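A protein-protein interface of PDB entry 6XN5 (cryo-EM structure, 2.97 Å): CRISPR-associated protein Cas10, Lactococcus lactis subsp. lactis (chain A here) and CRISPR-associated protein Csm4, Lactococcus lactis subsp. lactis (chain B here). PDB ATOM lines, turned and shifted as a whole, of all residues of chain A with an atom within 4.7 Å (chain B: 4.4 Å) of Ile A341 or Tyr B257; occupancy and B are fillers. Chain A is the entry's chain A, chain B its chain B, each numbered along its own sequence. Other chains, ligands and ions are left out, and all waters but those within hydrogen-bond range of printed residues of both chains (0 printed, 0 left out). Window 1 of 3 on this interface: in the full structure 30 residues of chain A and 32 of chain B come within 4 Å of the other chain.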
ATOM      1  N   PHE A 339      12.216  20.450 -24.159  1.00  0.00           N
ATOM      2  CA  PHE A 339      12.134  20.747 -25.583  1.00  0.00           C
ATOM      3  C   PHE A 339      11.049  21.800 -25.754  1.00  0.00           C
ATOM      4  O   PHE A 339       9.873  21.444 -25.847  1.00  0.00           O
ATOM      5  CB  PHE A 339      11.757  19.505 -26.381  1.00  0.00           C
ATOM      6  CG  PHE A 339      12.501  18.267 -25.995  1.00  0.00           C
ATOM      7  CD1 PHE A 339      13.769  18.019 -26.473  1.00  0.00           C
ATOM      8  CD2 PHE A 339      11.908  17.335 -25.164  1.00  0.00           C
ATOM      9  CE1 PHE A 339      14.426  16.865 -26.129  1.00  0.00           C
ATOM     10  CE2 PHE A 339      12.570  16.189 -24.808  1.00  0.00           C
ATOM     11  CZ  PHE A 339      13.832  15.956 -25.288  1.00  0.00           C
ATOM     12  N   LYS A 340      11.453  23.068 -25.886  1.00  0.00           N
ATOM     13  CA  LYS A 340      10.571  24.206 -25.619  1.00  0.00           C
ATOM     14  C   LYS A 340       9.335  24.227 -26.519  1.00  0.00           C
ATOM     15  O   LYS A 340       8.202  24.273 -26.035  1.00  0.00           O
ATOM     16  CB  LYS A 340      11.365  25.502 -25.772  1.00  0.00           C
ATOM     17  CG  LYS A 340      12.460  25.682 -24.750  1.00  0.00           C
ATOM     18  CD  LYS A 340      11.861  26.068 -23.421  1.00  0.00           C
ATOM     19  CE  LYS A 340      12.927  26.325 -22.388  1.00  0.00           C
ATOM     20  NZ  LYS A 340      13.589  27.639 -22.616  1.00  0.00           N
ATOM     21  N   ILE A 341       9.529  24.158 -27.828  1.00  0.00           N
ATOM     22  CA  ILE A 341       8.420  24.104 -28.774  1.00  0.00           C
ATOM     23  C   ILE A 341       8.657  22.872 -29.631  1.00  0.00           C
ATOM     24  O   ILE A 341       7.722  22.282 -30.186  1.00  0.00           O
ATOM     25  CB  ILE A 341       8.336  25.402 -29.607  1.00  0.00           C
ATOM     26  CG1 ILE A 341       8.028  26.589 -28.711  1.00  0.00           C
ATOM     27  CG2 ILE A 341       7.250  25.371 -30.666  1.00  0.00           C
ATOM     28  CD1 ILE A 341       6.721  26.481 -27.982  1.00  0.00           C
ATOM     29  N   ASP A 342       9.910  22.421 -29.651  1.00  0.00           N
ATOM     30  CA  ASP A 342      10.382  21.454 -30.630  1.00  0.00           C
ATOM     31  C   ASP A 342       9.778  20.068 -30.468  1.00  0.00           C
ATOM     32  O   ASP A 342       9.863  19.269 -31.403  1.00  0.00           O
ATOM     33  CB  ASP A 342      11.901  21.364 -30.554  1.00  0.00           C
ATOM     34  CG  ASP A 342      12.571  22.699 -30.792  1.00  0.00           C
ATOM     35  OD1 ASP A 342      11.954  23.567 -31.439  1.00  0.00           O
ATOM     36  OD2 ASP A 342      13.718  22.881 -30.335  1.00  0.00           O
ATOM     37  N   LEU A 343       9.166  19.765 -29.330  1.00  0.00           N
ATOM     38  CA  LEU A 343       8.484  18.496 -29.143  1.00  0.00           C
ATOM     39  C   LEU A 343       7.202  18.713 -28.360  1.00  0.00           C
ATOM     40  O   LEU A 343       7.169  19.505 -27.419  1.00  0.00           O
ATOM     41  CB  LEU A 343       9.369  17.489 -28.415  1.00  0.00           C
ATOM     42  CG  LEU A 343      10.254  16.646 -29.320  1.00  0.00           C
ATOM     43  CD1 LEU A 343      11.300  15.957 -28.497  1.00  0.00           C
ATOM     44  CD2 LEU A 343       9.414  15.646 -30.068  1.00  0.00           C
ATOM     45  N   TYR A 383      -0.776  25.165 -26.169  1.00  0.00           N
ATOM     46  CA  TYR A 383      -0.370  25.600 -24.843  1.00  0.00           C
ATOM     47  C   TYR A 383      -1.441  26.482 -24.221  1.00  0.00           C
ATOM     48  O   TYR A 383      -2.371  26.941 -24.886  1.00  0.00           O
ATOM     49  CB  TYR A 383       0.962  26.354 -24.896  1.00  0.00           C
ATOM     50  CG  TYR A 383       2.005  25.659 -25.726  1.00  0.00           C
ATOM     51  CD1 TYR A 383       2.688  24.558 -25.233  1.00  0.00           C
ATOM     52  CD2 TYR A 383       2.295  26.093 -27.005  1.00  0.00           C
ATOM     53  CE1 TYR A 383       3.632  23.913 -25.994  1.00  0.00           C
ATOM     54  CE2 TYR A 383       3.239  25.454 -27.772  1.00  0.00           C
ATOM     55  CZ  TYR A 383       3.903  24.365 -27.259  1.00  0.00           C
ATOM     56  OH  TYR A 383       4.846  23.723 -28.021  1.00  0.00           O
ATOM     57  N   LEU A 391       7.238  30.611 -20.987  1.00  0.00           N
ATOM     58  CA  LEU A 391       8.170  30.523 -22.106  1.00  0.00           C
ATOM     59  C   LEU A 391       8.835  31.862 -22.369  1.00  0.00           C
ATOM     60  O   LEU A 391      10.046  31.938 -22.596  1.00  0.00           O
ATOM     61  CB  LEU A 391       7.444  30.055 -23.361  1.00  0.00           C
ATOM     62  CG  LEU A 391       7.340  28.561 -23.616  1.00  0.00           C
ATOM     63  CD1 LEU A 391       6.360  28.329 -24.734  1.00  0.00           C
ATOM     64  CD2 LEU A 391       8.693  27.997 -23.964  1.00  0.00           C
ATOM     65  N   ASN A 392       8.049  32.934 -22.359  1.00  0.00           N
ATOM     66  CA  ASN A 392       8.604  34.252 -22.622  1.00  0.00           C
ATOM     67  C   ASN A 392       9.331  34.823 -21.417  1.00  0.00           C
ATOM     68  O   ASN A 392      10.094  35.780 -21.567  1.00  0.00           O
ATOM     69  CB  ASN A 392       7.495  35.197 -23.062  1.00  0.00           C
ATOM     70  CG  ASN A 392       6.912  34.817 -24.392  1.00  0.00           C
ATOM     71  OD1 ASN A 392       7.630  34.422 -25.301  1.00  0.00           O
ATOM     72  ND2 ASN A 392       5.602  34.911 -24.511  1.00  0.00           N
ATOM     73  N   LEU B 217       2.527  38.552 -30.711  1.00  0.00           N
ATOM     74  CA  LEU B 217       2.450  38.020 -29.361  1.00  0.00           C
ATOM     75  C   LEU B 217       1.715  39.026 -28.490  1.00  0.00           C
ATOM     76  O   LEU B 217       2.198  40.150 -28.308  1.00  0.00           O
ATOM     77  CB  LEU B 217       3.845  37.751 -28.804  1.00  0.00           C
ATOM     78  CG  LEU B 217       3.957  37.356 -27.337  1.00  0.00           C
ATOM     79  CD1 LEU B 217       3.266  36.037 -27.090  1.00  0.00           C
ATOM     80  CD2 LEU B 217       5.412  37.282 -26.940  1.00  0.00           C
ATOM     81  N   LEU B 234       2.978  28.470 -32.049  1.00  0.00           N
ATOM     82  CA  LEU B 234       4.054  29.269 -31.487  1.00  0.00           C
ATOM     83  C   LEU B 234       5.312  29.122 -32.330  1.00  0.00           C
ATOM     84  O   LEU B 234       5.586  28.063 -32.898  1.00  0.00           O
ATOM     85  CB  LEU B 234       4.331  28.845 -30.049  1.00  0.00           C
ATOM     86  CG  LEU B 234       3.701  29.698 -28.957  1.00  0.00           C
ATOM     87  CD1 LEU B 234       4.111  29.185 -27.607  1.00  0.00           C
ATOM     88  CD2 LEU B 234       4.136  31.120 -29.116  1.00  0.00           C
ATOM     89  N   GLU B 235       6.080  30.201 -32.422  1.00  0.00           N
ATOM     90  CA  GLU B 235       7.323  30.186 -33.173  1.00  0.00           C
ATOM     91  C   GLU B 235       8.399  30.904 -32.382  1.00  0.00           C
ATOM     92  O   GLU B 235       8.225  32.064 -32.007  1.00  0.00           O
ATOM     93  CB  GLU B 235       7.144  30.839 -34.538  1.00  0.00           C
ATOM     94  CG  GLU B 235       8.381  30.785 -35.400  1.00  0.00           C
ATOM     95  CD  GLU B 235       8.162  31.392 -36.764  1.00  0.00           C
ATOM     96  OE1 GLU B 235       7.043  31.874 -37.027  1.00  0.00           O
ATOM     97  OE2 GLU B 235       9.108  31.387 -37.577  1.00  0.00           O
ATOM     98  N   ARG B 236       9.509  30.215 -32.136  1.00  0.00           N
ATOM     99  CA  ARG B 236      10.646  30.813 -31.452  1.00  0.00           C
ATOM    100  C   ARG B 236      11.366  31.768 -32.389  1.00  0.00           C
ATOM    101  O   ARG B 236      11.818  31.371 -33.467  1.00  0.00           O
ATOM    102  CB  ARG B 236      11.608  29.732 -30.975  1.00  0.00           C
ATOM    103  CG  ARG B 236      12.654  30.220 -30.010  1.00  0.00           C
ATOM    104  CD  ARG B 236      13.851  29.296 -30.028  1.00  0.00           C
ATOM    105  NE  ARG B 236      14.569  29.399 -31.291  1.00  0.00           N
ATOM    106  CZ  ARG B 236      15.505  30.303 -31.549  1.00  0.00           C
ATOM    107  NH1 ARG B 236      15.856  31.185 -30.626  1.00  0.00           N
ATOM    108  NH2 ARG B 236      16.096  30.326 -32.729  1.00  0.00           N
ATOM    109  N   ASP B 255      15.036  35.093 -26.154  1.00  0.00           N
ATOM    110  CA  ASP B 255      14.148  34.302 -26.990  1.00  0.00           C
ATOM    111  C   ASP B 255      12.711  34.749 -26.785  1.00  0.00           C
ATOM    112  O   ASP B 255      12.227  34.808 -25.652  1.00  0.00           O
ATOM    113  CB  ASP B 255      14.283  32.820 -26.661  1.00  0.00           C
ATOM    114  CG  ASP B 255      15.278  32.118 -27.543  1.00  0.00           C
ATOM    115  OD1 ASP B 255      15.981  32.803 -28.312  1.00  0.00           O
ATOM    116  OD2 ASP B 255      15.365  30.878 -27.462  1.00  0.00           O
ATOM    117  N   LEU B 256      12.031  35.064 -27.878  1.00  0.00           N
ATOM    118  CA  LEU B 256      10.646  35.503 -27.833  1.00  0.00           C
ATOM    119  C   LEU B 256       9.815  34.539 -28.653  1.00  0.00           C
ATOM    120  O   LEU B 256      10.113  34.302 -29.826  1.00  0.00           O
ATOM    121  CB  LEU B 256      10.500  36.922 -28.365  1.00  0.00           C
ATOM    122  CG  LEU B 256       9.166  37.524 -27.963  1.00  0.00           C
ATOM    123  CD1 LEU B 256       9.190  37.823 -26.488  1.00  0.00           C
ATOM    124  CD2 LEU B 256       8.890  38.769 -28.745  1.00  0.00           C
ATOM    125  N   TYR B 257       8.778  33.991 -28.040  1.00  0.00           N
ATOM    126  CA  TYR B 257       7.913  33.010 -28.673  1.00  0.00           C
ATOM    127  C   TYR B 257       6.648  33.724 -29.111  1.00  0.00           C
ATOM    128  O   TYR B 257       5.800  34.055 -28.282  1.00  0.00           O
ATOM    129  CB  TYR B 257       7.580  31.869 -27.719  1.00  0.00           C
ATOM    130  CG  TYR B 257       8.760  31.060 -27.254  1.00  0.00           C
ATOM    131  CD1 TYR B 257       9.529  31.472 -26.180  1.00  0.00           C
ATOM    132  CD2 TYR B 257       9.094  29.879 -27.877  1.00  0.00           C
ATOM    133  CE1 TYR B 257      10.598  30.731 -25.748  1.00  0.00           C
ATOM    134  CE2 TYR B 257      10.164  29.134 -27.455  1.00  0.00           C
ATOM    135  CZ  TYR B 257      10.911  29.562 -26.392  1.00  0.00           C
ATOM    136  OH  TYR B 257      11.982  28.813 -25.970  1.00  0.00           O
ATOM    137  N   VAL B 258       6.521  33.962 -30.409  1.00  0.00           N
ATOM    138  CA  VAL B 258       5.367  34.644 -30.958  1.00  0.00           C
ATOM    139  C   VAL B 258       4.517  33.632 -31.716  1.00  0.00           C
ATOM    140  O   VAL B 258       4.938  32.510 -31.987  1.00  0.00           O
ATOM    141  CB  VAL B 258       5.774  35.818 -31.864  1.00  0.00           C
ATOM    142  CG1 VAL B 258       6.737  36.722 -31.142  1.00  0.00           C
ATOM    143  CG2 VAL B 258       6.390  35.304 -33.137  1.00  0.00           C
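The side-chain amide oxygen (OD1) of Asn A392 is in hydrogen-bond range of the backbone NH (N) of Tyr B257 (3.0 Å).
Of the 8 printed residues of chain B, 4 touch a printed residue of chain A. Hydrophobic or aromatic side chains of chain B within 4 Å of the printed part of chain A: Leu B217, Leu B234, Leu B256 and Tyr B257. Along chain B the printed residues that touch a printed residue of chain A span positions 217 to 257. Among the printed residues, 9 pairs touch across the chains. Among the printed residues, no Asp or Glu carboxylate lies within 4 Å of a Lys or Arg side-chain nitrogen of the other chain.
Among the printed residues, pairs that only touch across the chains: Lys A340 with Tyr B257, Asn A392 with Leu B217, Leu A391 with Tyr B257, Ile A341 with Tyr B257, Tyr A383 with Leu B234, Leu A391 with Leu B234, Ile A341 with Leu B234 and Asn A392 with Leu B256.
Of chain B, only Leu B234 (3.8 Å) and Tyr B257 (3.6 Å) come within 4 Å of Ile A341. Tyr B257 touches four residues of chain A. Printed residues of chain A within 4 Å of Leu B234: Ile A341 (3.8 Å), Tyr A383 (3.6 Å) and Leu A391 (3.7 Å). Printed residues of chain B within 4 Å of Leu A391: Leu B234 (3.7 Å) and Tyr B257 (3.4 Å). Of the printed residues of chain B, Tyr A383 touches Leu B234. Asp A342 touches none of the printed residues of chain B. The nearest printed residue of chain B that does not touch Ile A341 is Arg B236 (5.2 Å). The nearest printed residue of chain A that does not touch Leu B234 is Asn A392 (6.1 Å).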
